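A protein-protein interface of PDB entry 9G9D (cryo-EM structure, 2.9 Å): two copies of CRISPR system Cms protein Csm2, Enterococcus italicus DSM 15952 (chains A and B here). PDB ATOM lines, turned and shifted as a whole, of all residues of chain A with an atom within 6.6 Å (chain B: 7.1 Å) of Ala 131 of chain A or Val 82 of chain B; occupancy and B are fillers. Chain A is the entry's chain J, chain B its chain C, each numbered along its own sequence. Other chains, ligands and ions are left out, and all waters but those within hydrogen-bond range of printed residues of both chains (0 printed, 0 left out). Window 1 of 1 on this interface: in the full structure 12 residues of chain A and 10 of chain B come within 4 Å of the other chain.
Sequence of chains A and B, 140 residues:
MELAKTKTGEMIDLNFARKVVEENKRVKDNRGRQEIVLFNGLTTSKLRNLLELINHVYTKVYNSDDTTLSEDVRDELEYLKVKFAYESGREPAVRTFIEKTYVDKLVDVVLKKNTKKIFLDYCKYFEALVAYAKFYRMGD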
ATOM      1  N   LEU A  14     -12.165  -6.992  17.604  1.00  0.00           N
ATOM      2  CA  LEU A  14     -11.726  -7.180  16.198  1.00  0.00           C
ATOM      3  C   LEU A  14     -12.905  -7.780  15.425  1.00  0.00           C
ATOM      4  O   LEU A  14     -13.084  -7.435  14.244  1.00  0.00           O
ATOM      5  CB  LEU A  14     -10.498  -8.085  16.142  1.00  0.00           C
ATOM      6  CG  LEU A  14      -9.274  -7.643  16.952  1.00  0.00           C
ATOM      7  CD1 LEU A  14      -9.055  -6.140  16.986  1.00  0.00           C
ATOM      8  CD2 LEU A  14      -9.222  -8.242  18.347  1.00  0.00           C
ATOM      9  N   ASN A  15     -13.683  -8.643  16.078  1.00  0.00           N
ATOM     10  CA  ASN A  15     -14.896  -9.198  15.416  1.00  0.00           C
ATOM     11  C   ASN A  15     -15.830  -8.027  15.102  1.00  0.00           C
ATOM     12  O   ASN A  15     -16.362  -7.975  13.974  1.00  0.00           O
ATOM     13  CB  ASN A  15     -15.532 -10.286  16.270  1.00  0.00           C
ATOM     14  CG  ASN A  15     -14.567 -11.417  16.536  1.00  0.00           C
ATOM     15  OD1 ASN A  15     -13.443 -11.409  16.020  1.00  0.00           O
ATOM     16  ND2 ASN A  15     -14.983 -12.398  17.323  1.00  0.00           N
ATOM     17  N   ALA A  17     -14.881  -5.046  14.622  1.00  0.00           N
ATOM     18  CA  ALA A  17     -14.260  -4.323  13.516  1.00  0.00           C
ATOM     19  C   ALA A  17     -14.684  -4.910  12.176  1.00  0.00           C
ATOM     20  O   ALA A  17     -14.992  -4.170  11.230  1.00  0.00           O
ATOM     21  CB  ALA A  17     -12.738  -4.343  13.657  1.00  0.00           C
ATOM     22  N   LEU A  51      -4.055   5.230   9.857  1.00  0.00           N
ATOM     23  CA  LEU A  51      -3.261   4.169  10.525  1.00  0.00           C
ATOM     24  C   LEU A  51      -1.894   4.759  10.903  1.00  0.00           C
ATOM     25  O   LEU A  51      -1.472   4.575  12.055  1.00  0.00           O
ATOM     26  CB  LEU A  51      -3.113   2.920   9.657  1.00  0.00           C
ATOM     27  CG  LEU A  51      -2.434   1.726  10.333  1.00  0.00           C
ATOM     28  CD1 LEU A  51      -3.213   1.287  11.561  1.00  0.00           C
ATOM     29  CD2 LEU A  51      -2.263   0.570   9.366  1.00  0.00           C
ATOM     30  N   LYS A 124      -4.629  -1.979  18.012  1.00  0.00           N
ATOM     31  CA  LYS A 124      -4.975  -3.270  17.365  1.00  0.00           C
ATOM     32  C   LYS A 124      -6.344  -3.150  16.682  1.00  0.00           C
ATOM     33  O   LYS A 124      -6.488  -3.664  15.559  1.00  0.00           O
ATOM     34  CB  LYS A 124      -5.017  -4.405  18.391  1.00  0.00           C
ATOM     35  CG  LYS A 124      -3.684  -4.734  19.038  1.00  0.00           C
ATOM     36  CD  LYS A 124      -3.797  -5.806  20.114  1.00  0.00           C
ATOM     37  CE  LYS A 124      -2.477  -6.103  20.748  1.00  0.00           C
ATOM     38  NZ  LYS A 124      -2.585  -7.193  21.720  1.00  0.00           N
ATOM     39  N   PHE A 126      -7.705  -0.426  15.529  1.00  0.00           N
ATOM     40  CA  PHE A 126      -7.488   0.417  14.325  1.00  0.00           C
ATOM     41  C   PHE A 126      -6.820  -0.420  13.245  1.00  0.00           C
ATOM     42  O   PHE A 126      -7.223  -0.333  12.069  1.00  0.00           O
ATOM     43  CB  PHE A 126      -6.607   1.612  14.689  1.00  0.00           C
ATOM     44  CG  PHE A 126      -6.935   2.875  13.908  1.00  0.00           C
ATOM     45  CD1 PHE A 126      -6.399   3.092  12.645  1.00  0.00           C
ATOM     46  CD2 PHE A 126      -7.799   3.829  14.431  1.00  0.00           C
ATOM     47  CE1 PHE A 126      -6.710   4.238  11.934  1.00  0.00           C
ATOM     48  CE2 PHE A 126      -8.101   4.976  13.716  1.00  0.00           C
ATOM     49  CZ  PHE A 126      -7.558   5.177  12.471  1.00  0.00           C
ATOM     50  N   GLU A 127      -5.837  -1.236  13.641  1.00  0.00           N
ATOM     51  CA  GLU A 127      -5.116  -2.098  12.671  1.00  0.00           C
ATOM     52  C   GLU A 127      -6.104  -3.101  12.062  1.00  0.00           C
ATOM     53  O   GLU A 127      -6.056  -3.324  10.834  1.00  0.00           O
ATOM     54  CB  GLU A 127      -3.965  -2.803  13.387  1.00  0.00           C
ATOM     55  CG  GLU A 127      -3.285  -3.877  12.544  1.00  0.00           C
ATOM     56  CD  GLU A 127      -3.779  -5.290  12.790  1.00  0.00           C
ATOM     57  OE1 GLU A 127      -4.598  -5.483  13.713  1.00  0.00           O
ATOM     58  OE2 GLU A 127      -3.356  -6.198  12.042  1.00  0.00           O
ATOM     59  N   ALA A 128      -6.983  -3.656  12.897  1.00  0.00           N
ATOM     60  CA  ALA A 128      -7.975  -4.631  12.400  1.00  0.00           C
ATOM     61  C   ALA A 128      -8.814  -3.942  11.333  1.00  0.00           C
ATOM     62  O   ALA A 128      -8.951  -4.482  10.218  1.00  0.00           O
ATOM     63  CB  ALA A 128      -8.837  -5.129  13.533  1.00  0.00           C
ATOM     64  N   LEU A 129      -9.339  -2.763  11.668  1.00  0.00           N
ATOM     65  CA  LEU A 129     -10.204  -2.071  10.717  1.00  0.00           C
ATOM     66  C   LEU A 129      -9.507  -1.923   9.372  1.00  0.00           C
ATOM     67  O   LEU A 129     -10.096  -2.189   8.317  1.00  0.00           O
ATOM     68  CB  LEU A 129     -10.598  -0.700  11.262  1.00  0.00           C
ATOM     69  CG  LEU A 129     -11.531  -0.622  12.466  1.00  0.00           C
ATOM     70  CD1 LEU A 129     -11.553   0.798  12.990  1.00  0.00           C
ATOM     71  CD2 LEU A 129     -12.926  -1.062  12.077  1.00  0.00           C
ATOM     72  N   VAL A 130      -8.237  -1.512   9.399  1.00  0.00           N
ATOM     73  CA  VAL A 130      -7.476  -1.358   8.160  1.00  0.00           C
ATOM     74  C   VAL A 130      -7.366  -2.693   7.430  1.00  0.00           C
ATOM     75  O   VAL A 130      -7.559  -2.776   6.209  1.00  0.00           O
ATOM     76  CB  VAL A 130      -6.088  -0.764   8.454  1.00  0.00           C
ATOM     77  CG1 VAL A 130      -5.246  -0.732   7.188  1.00  0.00           C
ATOM     78  CG2 VAL A 130      -6.226   0.624   9.049  1.00  0.00           C
ATOM     79  N   ALA A 131      -7.031  -3.749   8.173  1.00  0.00           N
ATOM     80  CA  ALA A 131      -6.838  -5.075   7.536  1.00  0.00           C
ATOM     81  C   ALA A 131      -8.148  -5.526   6.896  1.00  0.00           C
ATOM     82  O   ALA A 131      -8.145  -5.911   5.710  1.00  0.00           O
ATOM     83  CB  ALA A 131      -6.362  -6.070   8.565  1.00  0.00           C
ATOM     84  N   TYR A 132      -9.234  -5.487   7.668  1.00  0.00           N
ATOM     85  CA  TYR A 132     -10.561  -5.904   7.144  1.00  0.00           C
ATOM     86  C   TYR A 132     -10.878  -5.109   5.881  1.00  0.00           C
ATOM     87  O   TYR A 132     -11.286  -5.710   4.867  1.00  0.00           O
ATOM     88  CB  TYR A 132     -11.574  -5.702   8.270  1.00  0.00           C
ATOM     89  CG  TYR A 132     -11.488  -6.775   9.344  1.00  0.00           C
ATOM     90  CD1 TYR A 132     -11.277  -8.105   9.008  1.00  0.00           C
ATOM     91  CD2 TYR A 132     -11.574  -6.450  10.691  1.00  0.00           C
ATOM     92  CE1 TYR A 132     -11.184  -9.088   9.979  1.00  0.00           C
ATOM     93  CE2 TYR A 132     -11.478  -7.423  11.670  1.00  0.00           C
ATOM     94  CZ  TYR A 132     -11.288  -8.745  11.314  1.00  0.00           C
ATOM     95  OH  TYR A 132     -11.198  -9.708  12.277  1.00  0.00           O
ATOM     96  N   ALA A 133     -10.688  -3.787   5.933  1.00  0.00           N
ATOM     97  CA  ALA A 133     -10.973  -2.970   4.759  1.00  0.00           C
ATOM     98  C   ALA A 133     -10.155  -3.434   3.562  1.00  0.00           C
ATOM     99  O   ALA A 133     -10.668  -3.517   2.440  1.00  0.00           O
ATOM    100  CB  ALA A 133     -10.697  -1.499   5.065  1.00  0.00           C
ATOM    101  N   LYS A 134      -8.875  -3.745   3.784  1.00  0.00           N
ATOM    102  CA  LYS A 134      -8.043  -4.257   2.700  1.00  0.00           C
ATOM    103  C   LYS A 134      -8.551  -5.606   2.203  1.00  0.00           C
ATOM    104  O   LYS A 134      -8.524  -5.885   0.999  1.00  0.00           O
ATOM    105  CB  LYS A 134      -6.591  -4.370   3.163  1.00  0.00           C
ATOM    106  CG  LYS A 134      -5.624  -4.775   2.068  1.00  0.00           C
ATOM    107  CD  LYS A 134      -5.735  -3.839   0.879  1.00  0.00           C
ATOM    108  CE  LYS A 134      -4.690  -4.152  -0.173  1.00  0.00           C
ATOM    109  NZ  LYS A 134      -3.314  -3.925   0.340  1.00  0.00           N
ATOM    110  N   PHE A 135      -9.018  -6.456   3.121  1.00  0.00           N
ATOM    111  CA  PHE A 135      -9.492  -7.783   2.740  1.00  0.00           C
ATOM    112  C   PHE A 135     -10.770  -7.710   1.915  1.00  0.00           C
ATOM    113  O   PHE A 135     -10.889  -8.387   0.888  1.00  0.00           O
ATOM    114  CB  PHE A 135      -9.711  -8.635   3.990  1.00  0.00           C
ATOM    115  CG  PHE A 135     -10.503  -9.886   3.741  1.00  0.00           C
ATOM    116  CD1 PHE A 135     -10.001 -10.892   2.934  1.00  0.00           C
ATOM    117  CD2 PHE A 135     -11.745 -10.062   4.326  1.00  0.00           C
ATOM    118  CE1 PHE A 135     -10.727 -12.044   2.705  1.00  0.00           C
ATOM    119  CE2 PHE A 135     -12.475 -11.214   4.103  1.00  0.00           C
ATOM    120  CZ  PHE A 135     -11.964 -12.206   3.291  1.00  0.00           C
ATOM    121  N   TYR A 136     -11.736  -6.898   2.344  1.00  0.00           N
ATOM    122  CA  TYR A 136     -13.015  -6.820   1.650  1.00  0.00           C
ATOM    123  C   TYR A 136     -12.948  -6.030   0.352  1.00  0.00           C
ATOM    124  O   TYR A 136     -13.842  -6.178  -0.488  1.00  0.00           O
ATOM    125  CB  TYR A 136     -14.078  -6.208   2.564  1.00  0.00           C
ATOM    126  CG  TYR A 136     -14.651  -7.182   3.567  1.00  0.00           C
ATOM    127  CD1 TYR A 136     -15.675  -8.048   3.211  1.00  0.00           C
ATOM    128  CD2 TYR A 136     -14.170  -7.236   4.865  1.00  0.00           C
ATOM    129  CE1 TYR A 136     -16.203  -8.941   4.122  1.00  0.00           C
ATOM    130  CE2 TYR A 136     -14.690  -8.126   5.783  1.00  0.00           C
ATOM    131  CZ  TYR A 136     -15.707  -8.975   5.406  1.00  0.00           C
ATOM    132  OH  TYR A 136     -16.229  -9.863   6.318  1.00  0.00           O
ATOM    133  N   GLU B  76      -4.000 -13.013  20.986  1.00  0.00           N
ATOM    134  CA  GLU B  76      -3.100 -13.313  19.842  1.00  0.00           C
ATOM    135  C   GLU B  76      -3.893 -14.081  18.775  1.00  0.00           C
ATOM    136  O   GLU B  76      -3.688 -13.807  17.580  1.00  0.00           O
ATOM    137  CB  GLU B  76      -1.870 -14.093  20.305  1.00  0.00           C
ATOM    138  CG  GLU B  76      -1.028 -13.329  21.319  1.00  0.00           C
ATOM    139  CD  GLU B  76      -0.811 -11.877  20.937  1.00  0.00           C
ATOM    140  OE1 GLU B  76      -0.201 -11.624  19.876  1.00  0.00           O
ATOM    141  OE2 GLU B  76      -1.262 -10.997  21.700  1.00  0.00           O
ATOM    142  N   LEU B  77      -4.745 -15.016  19.200  1.00  0.00           N
ATOM    143  CA  LEU B  77      -5.579 -15.781  18.238  1.00  0.00           C
ATOM    144  C   LEU B  77      -6.532 -14.825  17.501  1.00  0.00           C
ATOM    145  O   LEU B  77      -6.685 -14.972  16.270  1.00  0.00           O
ATOM    146  CB  LEU B  77      -6.338 -16.867  18.996  1.00  0.00           C
ATOM    147  CG  LEU B  77      -5.473 -17.971  19.610  1.00  0.00           C
ATOM    148  CD1 LEU B  77      -6.317 -18.975  20.370  1.00  0.00           C
ATOM    149  CD2 LEU B  77      -4.663 -18.658  18.526  1.00  0.00           C
ATOM    150  N   GLU B  78      -7.125 -13.865  18.213  1.00  0.00           N
ATOM    151  CA  GLU B  78      -7.991 -12.869  17.536  1.00  0.00           C
ATOM    152  C   GLU B  78      -7.141 -12.060  16.550  1.00  0.00           C
ATOM    153  O   GLU B  78      -7.602 -11.835  15.408  1.00  0.00           O
ATOM    154  CB  GLU B  78      -8.605 -11.953  18.592  1.00  0.00           C
ATOM    155  CG  GLU B  78      -9.808 -12.564  19.300  1.00  0.00           C
ATOM    156  CD  GLU B  78     -11.101 -12.349  18.537  1.00  0.00           C
ATOM    157  OE1 GLU B  78     -11.454 -11.172  18.310  1.00  0.00           O
ATOM    158  OE2 GLU B  78     -11.751 -13.349  18.166  1.00  0.00           O
ATOM    159  N   TYR B  79      -5.935 -11.677  16.969  1.00  0.00           N
ATOM    160  CA  TYR B  79      -5.030 -10.911  16.075  1.00  0.00           C
ATOM    161  C   TYR B  79      -4.657 -11.792  14.890  1.00  0.00           C
ATOM    162  O   TYR B  79      -4.532 -11.276  13.761  1.00  0.00           O
ATOM    163  CB  TYR B  79      -3.805 -10.452  16.868  1.00  0.00           C
ATOM    164  CG  TYR B  79      -3.068  -9.277  16.241  1.00  0.00           C
ATOM    165  CD1 TYR B  79      -3.436  -7.969  16.530  1.00  0.00           C
ATOM    166  CD2 TYR B  79      -2.013  -9.478  15.363  1.00  0.00           C
ATOM    167  CE1 TYR B  79      -2.772  -6.894  15.964  1.00  0.00           C
ATOM    168  CE2 TYR B  79      -1.342  -8.412  14.791  1.00  0.00           C
ATOM    169  CZ  TYR B  79      -1.724  -7.118  15.091  1.00  0.00           C
ATOM    170  OH  TYR B  79      -1.067  -6.065  14.527  1.00  0.00           O
ATOM    171  N   LEU B  80      -4.476 -13.094  15.134  1.00  0.00           N
ATOM    172  CA  LEU B  80      -4.049 -14.002  14.043  1.00  0.00           C
ATOM    173  C   LEU B  80      -5.128 -14.023  12.954  1.00  0.00           C
ATOM    174  O   LEU B  80      -4.766 -13.992  11.762  1.00  0.00           O
ATOM    175  CB  LEU B  80      -3.843 -15.384  14.659  1.00  0.00           C
ATOM    176  CG  LEU B  80      -3.342 -16.483  13.721  1.00  0.00           C
ATOM    177  CD1 LEU B  80      -1.959 -16.141  13.196  1.00  0.00           C
ATOM    178  CD2 LEU B  80      -3.323 -17.799  14.475  1.00  0.00           C
ATOM    179  N   LYS B  81      -6.400 -14.045  13.356  1.00  0.00           N
ATOM    180  CA  LYS B  81      -7.494 -14.028  12.355  1.00  0.00           C
ATOM    181  C   LYS B  81      -7.445 -12.717  11.557  1.00  0.00           C
ATOM    182  O   LYS B  81      -7.617 -12.772  10.321  1.00  0.00           O
ATOM    183  CB  LYS B  81      -8.853 -14.184  13.039  1.00  0.00           C
ATOM    184  CG  LYS B  81      -9.043 -15.521  13.727  1.00  0.00           C
ATOM    185  CD  LYS B  81     -10.506 -15.822  14.023  1.00  0.00           C
ATOM    186  CE  LYS B  81     -11.159 -14.706  14.769  1.00  0.00           C
ATOM    187  NZ  LYS B  81     -10.527 -14.503  16.073  1.00  0.00           N
ATOM    188  N   VAL B  82      -7.198 -11.593  12.234  1.00  0.00           N
ATOM    189  CA  VAL B  82      -7.098 -10.284  11.523  1.00  0.00           C
ATOM    190  C   VAL B  82      -5.910 -10.327  10.553  1.00  0.00           C
ATOM    191  O   VAL B  82      -6.066  -9.872   9.400  1.00  0.00           O
ATOM    192  CB  VAL B  82      -6.915  -9.156  12.552  1.00  0.00           C
ATOM    193  CG1 VAL B  82      -6.488  -7.847  11.904  1.00  0.00           C
ATOM    194  CG2 VAL B  82      -8.152  -8.964  13.417  1.00  0.00           C
ATOM    195  N   LYS B  83      -4.782 -10.889  10.996  1.00  0.00           N
ATOM    196  CA  LYS B  83      -3.581 -10.998  10.127  1.00  0.00           C
ATOM    197  C   LYS B  83      -3.898 -11.906   8.929  1.00  0.00           C
ATOM    198  O   LYS B  83      -3.466 -11.579   7.805  1.00  0.00           O
ATOM    199  CB  LYS B  83      -2.382 -11.479  10.951  1.00  0.00           C
ATOM    200  CG  LYS B  83      -1.585 -10.350  11.590  1.00  0.00           C
ATOM    201  CD  LYS B  83      -1.015  -9.400  10.542  1.00  0.00           C
ATOM    202  CE  LYS B  83      -0.113  -8.341  11.096  1.00  0.00           C
ATOM    203  NZ  LYS B  83      -0.842  -7.270  11.778  1.00  0.00           N
ATOM    204  N   PHE B  84      -4.620 -13.004   9.170  1.00  0.00           N
ATOM    205  CA  PHE B  84      -4.987 -13.924   8.061  1.00  0.00           C
ATOM    206  C   PHE B  84      -5.876 -13.179   7.073  1.00  0.00           C
ATOM    207  O   PHE B  84      -5.659 -13.305   5.852  1.00  0.00           O
ATOM    208  CB  PHE B  84      -5.712 -15.168   8.580  1.00  0.00           C
ATOM    209  CG  PHE B  84      -4.809 -16.234   9.186  1.00  0.00           C
ATOM    210  CD1 PHE B  84      -3.473 -16.328   8.816  1.00  0.00           C
ATOM    211  CD2 PHE B  84      -5.307 -17.155  10.100  1.00  0.00           C
ATOM    212  CE1 PHE B  84      -2.654 -17.304   9.360  1.00  0.00           C
ATOM    213  CE2 PHE B  84      -4.484 -18.132  10.636  1.00  0.00           C
ATOM    214  CZ  PHE B  84      -3.161 -18.204  10.267  1.00  0.00           C
ATOM    215  N   ALA B  85      -6.821 -12.385   7.586  1.00  0.00           N
ATOM    216  CA  ALA B  85      -7.712 -11.598   6.702  1.00  0.00           C
ATOM    217  C   ALA B  85      -6.876 -10.594   5.910  1.00  0.00           C
ATOM    218  O   ALA B  85      -7.105 -10.428   4.695  1.00  0.00           O
ATOM    219  CB  ALA B  85      -8.770 -10.902   7.524  1.00  0.00           C
ATOM    220  N   TYR B  86      -5.906  -9.971   6.579  1.00  0.00           N
ATOM    221  CA  TYR B  86      -5.065  -8.953   5.905  1.00  0.00           C
ATOM    222  C   TYR B  86      -4.323  -9.619   4.777  1.00  0.00           C
ATOM    223  O   TYR B  86      -4.397  -9.136   3.631  1.00  0.00           O
ATOM    224  CB  TYR B  86      -4.017  -8.370   6.855  1.00  0.00           C
ATOM    225  CG  TYR B  86      -3.259  -7.190   6.267  1.00  0.00           C
ATOM    226  CD1 TYR B  86      -3.918  -6.217   5.526  1.00  0.00           C
ATOM    227  CD2 TYR B  86      -1.884  -7.068   6.421  1.00  0.00           C
ATOM    228  CE1 TYR B  86      -3.238  -5.141   4.984  1.00  0.00           C
ATOM    229  CE2 TYR B  86      -1.192  -5.999   5.879  1.00  0.00           C
ATOM    230  CZ  TYR B  86      -1.871  -5.033   5.161  1.00  0.00           C
ATOM    231  OH  TYR B  86      -1.203  -3.975   4.618  1.00  0.00           O
ATOM    232  N   GLU B  87      -3.633 -10.720   5.080  1.00  0.00           N
ATOM    233  CA  GLU B  87      -2.799 -11.350   4.063  1.00  0.00           C
ATOM    234  C   GLU B  87      -3.644 -11.960   2.952  1.00  0.00           C
ATOM    235  O   GLU B  87      -3.219 -11.995   1.792  1.00  0.00           O
ATOM    236  CB  GLU B  87      -1.891 -12.399   4.701  1.00  0.00           C
ATOM    237  CG  GLU B  87      -0.776 -11.807   5.549  1.00  0.00           C
ATOM    238  CD  GLU B  87       0.166 -10.925   4.748  1.00  0.00           C
ATOM    239  OE1 GLU B  87       0.298 -11.143   3.525  1.00  0.00           O
ATOM    240  OE2 GLU B  87       0.778 -10.012   5.343  1.00  0.00           O
ATOM    241  N   SER B  88      -4.848 -12.416   3.294  1.00  0.00           N
ATOM    242  CA  SER B  88      -5.755 -12.920   2.235  1.00  0.00           C
ATOM    243  C   SER B  88      -5.966 -11.802   1.208  1.00  0.00           C
ATOM    244  O   SER B  88      -5.814 -12.069  -0.002  1.00  0.00           O
ATOM    245  CB  SER B  88      -7.060 -13.380   2.816  1.00  0.00           C
ATOM    246  OG  SER B  88      -6.855 -14.425   3.757  1.00  0.00           O
ATOM    247  N   GLY B  89      -6.310 -10.600   1.675  1.00  0.00           N
ATOM    248  CA  GLY B  89      -6.563  -9.463   0.768  1.00  0.00           C
ATOM    249  C   GLY B  89      -5.345  -9.040  -0.032  1.00  0.00           C
ATOM    250  O   GLY B  89      -5.515  -8.746  -1.233  1.00  0.00           O
ATOM    251  N   ASP B 104      -7.913 -20.300   9.124  1.00  0.00           N
ATOM    252  CA  ASP B 104      -8.637 -19.201   9.815  1.00  0.00           C
ATOM    253  C   ASP B 104      -9.811 -19.800  10.593  1.00  0.00           C
ATOM    254  O   ASP B 104     -10.035 -19.384  11.750  1.00  0.00           O
ATOM    255  CB  ASP B 104      -9.087 -18.132   8.835  1.00  0.00           C
ATOM    256  CG  ASP B 104      -9.545 -16.829   9.474  1.00  0.00           C
ATOM    257  OD1 ASP B 104      -8.713 -16.184  10.143  1.00  0.00           O
ATOM    258  OD2 ASP B 104     -10.731 -16.479   9.305  1.00  0.00           O
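The side-chain carboxylate of Glu 78 of chain B lies within salt-bridge range of the side-chain amino group of Lys 81 of chain B.
OH of Tyr 79 of chain B sits at hydrogen-bond distance from NZ of Lys 83 of chain B.
The side-chain hydroxyl (OG) of Ser 88 of chain B lies within hydrogen-bond range of the backbone carbonyl oxygen (O) of Phe 84 of chain B, at 2.7 Å.
The side-chain carboxylate (OE1) of Glu 78 of chain B lies close to the side-chain amide oxygen (OD1) of Asn 15 of chain A (3.0 Å).
OE2 of Glu 127 of chain A sits close to OH of Tyr 79 of chain B (3.4 Å).
The side-chain carboxylate of Glu 127 of chain A lies within salt-bridge range of the side-chain amino group of Lys 83 of chain B, at 2.7 Å.
Ala 131 of chain A touches two residues of chain B.
Of chain A, only Leu 14, Glu 127, Ala 128, Ala 131 and Tyr 132 come within 4 Å of Val 82 of chain B.
Of the printed residues of chain B, Phe 135 of chain A touches Ala 85 (3.2 Å), Ser 88 (3.9 Å) and Gly 89 (3.9 Å).
Printed residues of chain A within 4 Å of Ala 85 of chain B: Tyr 132 (3.9 Å) and Phe 135 (3.2 Å).
Printed residues of chain B within 4 Å of Lys 134 of chain A: Tyr 86.
Of the printed residues of chain B, Tyr 132 of chain A touches Val 82 (3.3 Å) and Ala 85 (3.9 Å).
The nearest residue of chain B that does not touch Ala 131 of chain A is Ala 85 of chain B (4.7 Å).
The nearest residue of chain A that does not touch Val 82 of chain B is Lys 124 of chain A (5.6 Å).
Val 82 of chain B touches Leu 14 of chain A.
Lys 124 of chain A touches Tyr 79 of chain B.
OE1 of Glu 127 of chain A touches CG1 of Val 82 of chain B, 3.5 Å away.
Tyr 86 of chain B touches Ala 131 of chain A.
Tyr 132 of chain A touches Val 82 of chain B (OH to CG2, 3.3 Å).
Tyr 132 of chain A touches Ala 85 of chain B (CE1 to CB, 3.9 Å).
CG of Lys 134 of chain A touches CE1 of Tyr 86 of chain B (3.8 Å).
CB of Phe 135 of chain A touches O of Ala 85 of chain B (3.2 Å).
CD1 of Phe 135 of chain A touches CB of Ser 88 of chain B, at 3.9 Å.
Phe 135 of chain A touches Gly 89 of chain B (CA to CA, 3.9 Å).
Hydrophobic or aromatic side chains of chain A within 4 Å of the printed part of chain B: Leu 14, Ala 128, Ala 131, Tyr 132 and Phe 135.
Printed residues of chain B that touch a printed residue of chain A: Glu 78, Tyr 79, Val 82, Lys 83, Ala 85, Tyr 86, Ser 88 and Gly 89.
Hydrophobic or aromatic side chains of chain B that line the printed part of chain A: Tyr 79, Val 82, Ala 85 and Tyr 86.
Among the printed residues, Asp or Glu carboxylates within 4 Å of a Lys or Arg side-chain nitrogen of the other chain: Glu 127 of chain A with Lys 83 of chain B (2.7 Å).
No position is printed for both chains.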
